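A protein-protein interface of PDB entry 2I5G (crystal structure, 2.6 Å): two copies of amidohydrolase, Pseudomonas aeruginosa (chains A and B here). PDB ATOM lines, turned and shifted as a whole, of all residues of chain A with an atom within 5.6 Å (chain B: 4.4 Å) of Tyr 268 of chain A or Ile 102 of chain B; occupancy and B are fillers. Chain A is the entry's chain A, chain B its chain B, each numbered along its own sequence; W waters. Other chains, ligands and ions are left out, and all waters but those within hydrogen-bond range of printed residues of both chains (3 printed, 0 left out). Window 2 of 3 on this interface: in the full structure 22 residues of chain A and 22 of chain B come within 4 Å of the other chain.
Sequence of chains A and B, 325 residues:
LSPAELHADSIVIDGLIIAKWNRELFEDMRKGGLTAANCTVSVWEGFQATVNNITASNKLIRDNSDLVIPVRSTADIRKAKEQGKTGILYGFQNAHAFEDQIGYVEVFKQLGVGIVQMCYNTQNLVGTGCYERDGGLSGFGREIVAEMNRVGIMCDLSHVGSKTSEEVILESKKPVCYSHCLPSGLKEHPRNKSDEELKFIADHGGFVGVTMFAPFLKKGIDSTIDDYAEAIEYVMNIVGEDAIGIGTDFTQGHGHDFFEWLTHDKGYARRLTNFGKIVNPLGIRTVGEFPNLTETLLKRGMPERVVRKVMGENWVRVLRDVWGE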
ATOM      1  N   TRP A  44      -6.966   2.979  10.379  1.00  0.00           N
ATOM      2  CA  TRP A  44      -7.008   4.113   9.456  1.00  0.00           C
ATOM      3  C   TRP A  44      -6.644   5.411  10.188  1.00  0.00           C
ATOM      4  O   TRP A  44      -6.223   6.388   9.565  1.00  0.00           O
ATOM      5  CB  TRP A  44      -8.407   4.269   8.841  1.00  0.00           C
ATOM      6  CG  TRP A  44      -8.797   3.252   7.782  1.00  0.00           C
ATOM      7  CD1 TRP A  44      -9.949   2.517   7.745  1.00  0.00           C
ATOM      8  CD2 TRP A  44      -8.071   2.909   6.590  1.00  0.00           C
ATOM      9  NE1 TRP A  44      -9.988   1.744   6.611  1.00  0.00           N
ATOM     10  CE2 TRP A  44      -8.851   1.963   5.883  1.00  0.00           C
ATOM     11  CE3 TRP A  44      -6.838   3.308   6.050  1.00  0.00           C
ATOM     12  CZ2 TRP A  44      -8.439   1.409   4.664  1.00  0.00           C
ATOM     13  CZ3 TRP A  44      -6.430   2.759   4.838  1.00  0.00           C
ATOM     14  CH2 TRP A  44      -7.231   1.818   4.159  1.00  0.00           C
ATOM     15  N   TRP A 261     -16.159  -0.160   7.094  1.00  0.00           N
ATOM     16  CA  TRP A 261     -15.059   0.723   7.459  1.00  0.00           C
ATOM     17  C   TRP A 261     -13.718   0.115   7.058  1.00  0.00           C
ATOM     18  O   TRP A 261     -12.784   0.816   6.669  1.00  0.00           O
ATOM     19  CB  TRP A 261     -15.093   0.950   8.967  1.00  0.00           C
ATOM     20  CG  TRP A 261     -14.053   1.871   9.464  1.00  0.00           C
ATOM     21  CD1 TRP A 261     -13.902   3.189   9.144  1.00  0.00           C
ATOM     22  CD2 TRP A 261     -13.041   1.571  10.427  1.00  0.00           C
ATOM     23  NE1 TRP A 261     -12.861   3.732   9.857  1.00  0.00           N
ATOM     24  CE2 TRP A 261     -12.315   2.760  10.652  1.00  0.00           C
ATOM     25  CE3 TRP A 261     -12.680   0.413  11.125  1.00  0.00           C
ATOM     26  CZ2 TRP A 261     -11.248   2.829  11.552  1.00  0.00           C
ATOM     27  CZ3 TRP A 261     -11.616   0.480  12.024  1.00  0.00           C
ATOM     28  CH2 TRP A 261     -10.917   1.683  12.227  1.00  0.00           C
ATOM     29  N   HIS A 264     -13.509   0.166   2.779  1.00  0.00           N
ATOM     30  CA  HIS A 264     -13.440   1.373   1.960  1.00  0.00           C
ATOM     31  C   HIS A 264     -12.141   2.097   2.299  1.00  0.00           C
ATOM     32  O   HIS A 264     -11.774   2.197   3.469  1.00  0.00           O
ATOM     33  CB  HIS A 264     -14.637   2.290   2.230  1.00  0.00           C
ATOM     34  CG  HIS A 264     -15.941   1.756   1.724  1.00  0.00           C
ATOM     35  ND1 HIS A 264     -16.608   0.711   2.330  1.00  0.00           N
ATOM     36  CD2 HIS A 264     -16.698   2.116   0.660  1.00  0.00           C
ATOM     37  CE1 HIS A 264     -17.718   0.451   1.660  1.00  0.00           C
ATOM     38  NE2 HIS A 264     -17.796   1.290   0.643  1.00  0.00           N
ATOM     39  N   ASP A 265     -11.437   2.589   1.283  1.00  0.00           N
ATOM     40  CA  ASP A 265     -10.175   3.292   1.516  1.00  0.00           C
ATOM     41  C   ASP A 265     -10.352   4.421   2.539  1.00  0.00           C
ATOM     42  O   ASP A 265     -11.303   5.201   2.455  1.00  0.00           O
ATOM     43  CB  ASP A 265      -9.633   3.863   0.197  1.00  0.00           C
ATOM     44  CG  ASP A 265      -8.231   4.451   0.341  1.00  0.00           C
ATOM     45  OD1 ASP A 265      -7.328   3.712   0.779  1.00  0.00           O
ATOM     46  OD2 ASP A 265      -8.032   5.645   0.012  1.00  0.00           O
ATOM     47  N   LYS A 266      -9.432   4.497   3.501  1.00  0.00           N
ATOM     48  CA  LYS A 266      -9.481   5.519   4.544  1.00  0.00           C
ATOM     49  C   LYS A 266     -10.656   5.274   5.480  1.00  0.00           C
ATOM     50  O   LYS A 266     -10.937   6.082   6.366  1.00  0.00           O
ATOM     51  CB  LYS A 266      -9.610   6.918   3.925  1.00  0.00           C
ATOM     52  CG  LYS A 266      -8.296   7.625   3.631  1.00  0.00           C
ATOM     53  CD  LYS A 266      -7.436   6.846   2.677  1.00  0.00           C
ATOM     54  CE  LYS A 266      -6.142   7.571   2.408  1.00  0.00           C
ATOM     55  NZ  LYS A 266      -5.420   6.902   1.300  1.00  0.00           N
ATOM     56  N   GLY A 267     -11.340   4.156   5.274  1.00  0.00           N
ATOM     57  CA  GLY A 267     -12.483   3.830   6.101  1.00  0.00           C
ATOM     58  C   GLY A 267     -13.773   4.475   5.629  1.00  0.00           C
ATOM     59  O   GLY A 267     -14.814   4.286   6.261  1.00  0.00           O
ATOM     60  N   TYR A 268     -13.723   5.216   4.522  1.00  0.00           N
ATOM     61  CA  TYR A 268     -14.921   5.885   4.017  1.00  0.00           C
ATOM     62  C   TYR A 268     -14.945   6.125   2.507  1.00  0.00           C
ATOM     63  O   TYR A 268     -16.007   6.348   1.937  1.00  0.00           O
ATOM     64  CB  TYR A 268     -15.097   7.239   4.721  1.00  0.00           C
ATOM     65  CG  TYR A 268     -14.222   8.333   4.145  1.00  0.00           C
ATOM     66  CD1 TYR A 268     -14.581   8.989   2.966  1.00  0.00           C
ATOM     67  CD2 TYR A 268     -12.998   8.655   4.730  1.00  0.00           C
ATOM     68  CE1 TYR A 268     -13.740   9.931   2.379  1.00  0.00           C
ATOM     69  CE2 TYR A 268     -12.145   9.598   4.153  1.00  0.00           C
ATOM     70  CZ  TYR A 268     -12.523  10.231   2.976  1.00  0.00           C
ATOM     71  OH  TYR A 268     -11.689  11.163   2.393  1.00  0.00           O
ATOM     72  N   ALA A 269     -13.784   6.111   1.863  1.00  0.00           N
ATOM     73  CA  ALA A 269     -13.711   6.371   0.424  1.00  0.00           C
ATOM     74  C   ALA A 269     -14.170   5.214  -0.451  1.00  0.00           C
ATOM     75  O   ALA A 269     -15.017   4.426  -0.056  1.00  0.00           O
ATOM     76  CB  ALA A 269     -12.294   6.779   0.043  1.00  0.00           C
ATOM     77  N   ARG A 270     -13.604   5.120  -1.647  1.00  0.00           N
ATOM     78  CA  ARG A 270     -13.970   4.073  -2.593  1.00  0.00           C
ATOM     79  C   ARG A 270     -13.906   2.655  -2.021  1.00  0.00           C
ATOM     80  O   ARG A 270     -13.150   2.367  -1.098  1.00  0.00           O
ATOM     81  CB  ARG A 270     -13.076   4.164  -3.829  1.00  0.00           C
ATOM     82  CG  ARG A 270     -11.630   3.889  -3.528  1.00  0.00           C
ATOM     83  CD  ARG A 270     -10.722   4.177  -4.710  1.00  0.00           C
ATOM     84  NE  ARG A 270      -9.345   3.845  -4.365  1.00  0.00           N
ATOM     85  CZ  ARG A 270      -8.668   4.439  -3.391  1.00  0.00           C
ATOM     86  NH1 ARG A 270      -9.242   5.402  -2.683  1.00  0.00           N
ATOM     87  NH2 ARG A 270      -7.432   4.043  -3.103  1.00  0.00           N
ATOM     88  N   ASP B 100      -6.260  12.806   4.731  1.00  0.00           N
ATOM     89  CA  ASP B 100      -7.030  11.715   4.137  1.00  0.00           C
ATOM     90  C   ASP B 100      -8.507  12.052   4.019  1.00  0.00           C
ATOM     91  O   ASP B 100      -9.365  11.175   4.102  1.00  0.00           O
ATOM     92  CB  ASP B 100      -6.853  10.431   4.952  1.00  0.00           C
ATOM     93  CG  ASP B 100      -7.404  10.542   6.360  1.00  0.00           C
ATOM     94  OD1 ASP B 100      -7.617  11.673   6.843  1.00  0.00           O
ATOM     95  OD2 ASP B 100      -7.608   9.488   6.993  1.00  0.00           O
ATOM     96  N   GLN B 101      -8.803  13.329   3.822  1.00  0.00           N
ATOM     97  CA  GLN B 101     -10.187  13.763   3.689  1.00  0.00           C
ATOM     98  C   GLN B 101     -10.434  14.431   2.350  1.00  0.00           C
ATOM     99  O   GLN B 101      -9.913  15.517   2.079  1.00  0.00           O
ATOM    100  CB  GLN B 101     -10.550  14.727   4.815  1.00  0.00           C
ATOM    101  CG  GLN B 101     -10.383  14.128   6.186  1.00  0.00           C
ATOM    102  CD  GLN B 101     -11.016  12.757   6.278  1.00  0.00           C
ATOM    103  OE1 GLN B 101     -12.214  12.591   6.020  1.00  0.00           O
ATOM    104  NE2 GLN B 101     -10.218  11.762   6.643  1.00  0.00           N
ATOM    105  N   ILE B 102     -11.225  13.773   1.509  1.00  0.00           N
ATOM    106  CA  ILE B 102     -11.557  14.316   0.203  1.00  0.00           C
ATOM    107  C   ILE B 102     -12.450  15.547   0.407  1.00  0.00           C
ATOM    108  O   ILE B 102     -12.551  16.414  -0.464  1.00  0.00           O
ATOM    109  CB  ILE B 102     -12.279  13.260  -0.656  1.00  0.00           C
ATOM    110  CG1 ILE B 102     -11.341  12.072  -0.897  1.00  0.00           C
ATOM    111  CG2 ILE B 102     -12.725  13.866  -1.980  1.00  0.00           C
ATOM    112  CD1 ILE B 102     -11.967  10.919  -1.689  1.00  0.00           C
ATOM    113  N   GLY B 103     -13.078  15.619   1.578  1.00  0.00           N
ATOM    114  CA  GLY B 103     -13.932  16.748   1.899  1.00  0.00           C
ATOM    115  C   GLY B 103     -13.165  18.027   2.194  1.00  0.00           C
ATOM    116  O   GLY B 103     -13.736  19.114   2.166  1.00  0.00           O
ATOM    117  N   TYR B 104     -11.871  17.905   2.479  1.00  0.00           N
ATOM    118  CA  TYR B 104     -11.040  19.070   2.768  1.00  0.00           C
ATOM    119  C   TYR B 104     -10.781  19.899   1.518  1.00  0.00           C
ATOM    120  O   TYR B 104     -10.488  21.095   1.604  1.00  0.00           O
ATOM    121  CB  TYR B 104      -9.704  18.635   3.360  1.00  0.00           C
ATOM    122  CG  TYR B 104      -9.778  18.215   4.805  1.00  0.00           C
ATOM    123  CD1 TYR B 104     -11.010  18.055   5.445  1.00  0.00           C
ATOM    124  CD2 TYR B 104      -8.617  17.929   5.526  1.00  0.00           C
ATOM    125  CE1 TYR B 104     -11.084  17.620   6.763  1.00  0.00           C
ATOM    126  CE2 TYR B 104      -8.683  17.490   6.839  1.00  0.00           C
ATOM    127  CZ  TYR B 104      -9.919  17.336   7.450  1.00  0.00           C
ATOM    128  OH  TYR B 104      -9.995  16.882   8.743  1.00  0.00           O
ATOM    129  N   VAL B 105     -10.868  19.256   0.357  1.00  0.00           N
ATOM    130  CA  VAL B 105     -10.654  19.954  -0.899  1.00  0.00           C
ATOM    131  C   VAL B 105     -11.643  21.118  -0.966  1.00  0.00           C
ATOM    132  O   VAL B 105     -11.253  22.281  -1.133  1.00  0.00           O
ATOM    133  CB  VAL B 105     -10.879  19.011  -2.091  1.00  0.00           C
ATOM    134  CG1 VAL B 105     -10.689  19.762  -3.393  1.00  0.00           C
ATOM    135  CG2 VAL B 105      -9.912  17.829  -1.999  1.00  0.00           C
ATOM    136  N   PHE B 140      -6.509   7.005  -4.145  1.00  0.00           N
ATOM    137  CA  PHE B 140      -6.912   8.149  -3.338  1.00  0.00           C
ATOM    138  C   PHE B 140      -6.597   9.434  -4.111  1.00  0.00           C
ATOM    139  O   PHE B 140      -7.319  10.425  -4.015  1.00  0.00           O
ATOM    140  CB  PHE B 140      -6.163   8.154  -2.007  1.00  0.00           C
ATOM    141  CG  PHE B 140      -6.571   9.267  -1.096  1.00  0.00           C
ATOM    142  CD1 PHE B 140      -7.841   9.288  -0.537  1.00  0.00           C
ATOM    143  CD2 PHE B 140      -5.689  10.300  -0.802  1.00  0.00           C
ATOM    144  CE1 PHE B 140      -8.230  10.326   0.307  1.00  0.00           C
ATOM    145  CE2 PHE B 140      -6.065  11.341   0.039  1.00  0.00           C
ATOM    146  CZ  PHE B 140      -7.337  11.355   0.594  1.00  0.00           C
ATOM    147  N   GLU B 143      -9.118  10.190  -6.730  1.00  0.00           N
ATOM    148  CA  GLU B 143     -10.337  10.753  -6.162  1.00  0.00           C
ATOM    149  C   GLU B 143     -10.114  12.240  -5.884  1.00  0.00           C
ATOM    150  O   GLU B 143     -10.990  13.070  -6.146  1.00  0.00           O
ATOM    151  CB  GLU B 143     -10.746  10.016  -4.874  1.00  0.00           C
ATOM    152  CG  GLU B 143     -11.135   8.549  -5.095  1.00  0.00           C
ATOM    153  CD  GLU B 143     -11.967   7.959  -3.957  1.00  0.00           C
ATOM    154  OE1 GLU B 143     -13.158   8.316  -3.830  1.00  0.00           O
ATOM    155  OE2 GLU B 143     -11.431   7.138  -3.186  1.00  0.00           O
ATOM    156  N   ILE B 144      -8.932  12.573  -5.376  1.00  0.00           N
ATOM    157  CA  ILE B 144      -8.612  13.957  -5.081  1.00  0.00           C
ATOM    158  C   ILE B 144      -8.681  14.828  -6.343  1.00  0.00           C
ATOM    159  O   ILE B 144      -9.281  15.906  -6.324  1.00  0.00           O
ATOM    160  CB  ILE B 144      -7.219  14.072  -4.454  1.00  0.00           C
ATOM    161  CG1 ILE B 144      -7.243  13.502  -3.036  1.00  0.00           C
ATOM    162  CG2 ILE B 144      -6.778  15.528  -4.432  1.00  0.00           C
ATOM    163  CD1 ILE B 144      -8.160  14.265  -2.079  1.00  0.00           C
ATOM    164  N   GLU B 147     -12.250  15.523  -7.366  1.00  0.00           N
ATOM    165  CA  GLU B 147     -12.888  16.498  -6.483  1.00  0.00           C
ATOM    166  C   GLU B 147     -12.347  17.903  -6.763  1.00  0.00           C
ATOM    167  O   GLU B 147     -13.106  18.879  -6.789  1.00  0.00           O
ATOM    168  CB  GLU B 147     -12.649  16.129  -5.015  1.00  0.00           C
ATOM    169  CG  GLU B 147     -13.354  17.050  -4.026  1.00  0.00           C
ATOM    170  CD  GLU B 147     -14.866  16.881  -4.027  1.00  0.00           C
ATOM    171  OE1 GLU B 147     -15.435  16.584  -5.096  1.00  0.00           O
ATOM    172  OE2 GLU B 147     -15.490  17.060  -2.961  1.00  0.00           O
HETATM  173  O   HOH W   1      -6.157   7.017   6.619  1.00  0.00           O
HETATM  174  O   HOH W   2      -4.996   5.042  -2.714  1.00  0.00           O
HETATM  175  O   HOH W   3     -13.646  13.479   3.754  1.00  0.00           O
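OH of Tyr 268 of chain A sits at hydrogen-bond distance from N of Ile 102 of chain B. The guanidinium group of Arg 270 of chain A lies within salt-bridge range of the side-chain carboxylate of Glu 143 of chain B (2.8 Å). The side-chain hydroxyl of Tyr 268 of chain A lies within hydrogen-bond range of the backbone carbonyl oxygen of Asp 100 of chain B (2.9 Å). The guanidinium group of Arg 270 of chain A sits close to the backbone NH of Phe 140 of chain B (3.3 Å).
The side-chain amide nitrogen of Gln 101 of chain B is in hydrogen-bond range of the side-chain carboxylate of Asp 100 of chain B (2.6 Å). OD2 of Asp 265 of chain A is in salt-bridge range of NZ of Lys 266 of chain A. OD2 of Asp 265 of chain A is in salt-bridge range of NH1 of Arg 270 of chain A (3.0 Å).
OD2 of Asp 265 of chain A touches CD1 of Phe 140 of chain B, 3.7 Å away. Lys 266 of chain A touches Asp 100 of chain B. Lys 266 of chain A touches Phe 140 of chain B (NZ to CG, 3.6 Å). OH of Tyr 268 of chain A touches CA of Gln 101 of chain B (3.3 Å). Ala 269 of chain A touches Glu 143 of chain B (CB to OE2, 3.4 Å).
His 264 of chain A touches none of the printed residues of chain B. Of the printed residues of chain B, Asp 265 of chain A touches Phe 140 (3.7 Å). Printed residues of chain B within 4 Å of Lys 266 of chain A: Asp 100 (3.4 Å) and Phe 140 (3.6 Å). Gly 267 of chain A touches none of the printed residues of chain B. Of the printed residues of chain B, Ala 269 of chain A touches Glu 143. Printed residues of chain B within 4 Å of Arg 270 of chain A: Phe 140 (3.3 Å) and Glu 143 (2.8 Å). Of chain A, only Tyr 268 comes within 4 Å of Ile 102 of chain B. Of the printed residues of chain A, Phe 140 of chain B touches Asp 265 (3.7 Å), Lys 266 (3.6 Å) and Arg 270 (3.3 Å). The nearest residue of chain B that does not touch Tyr 268 of chain A is Phe 140 of chain B (4.1 Å).
Printed residues of chain B that touch a printed residue of chain A: Asp 100, Gln 101, Ile 102, Phe 140 and Glu 143. Along chain A the printed residues that touch a printed residue of chain B span positions 265 to 270. Among the printed residues, 9 pairs touch across the chains. Among the printed residues, Asp or Glu carboxylates within 4 Å of a Lys or Arg side-chain nitrogen of the other chain: Arg 270 of chain A with Glu 143 of chain B (2.8 Å).
No position is printed for both chains. Of the 9 pairs that touch across the chains among the printed residues, none has its exchanged pair printed and touching as well.
Water W2 bridges NH2 of Arg 270 of chain A (2.7 Å) and N of Phe 140 of chain B (2.9 Å). Water W3 lies within hydrogen-bond range of OE1 of Gln 101 of chain B, N of Gly 103 of chain B, N of Ile 102 of chain B and OH of Tyr 268 of chain A. Water W1 bridges OD2 of Asp 100 of chain B (2.9 Å) and O of Trp 44 of chain A (3.0 Å).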
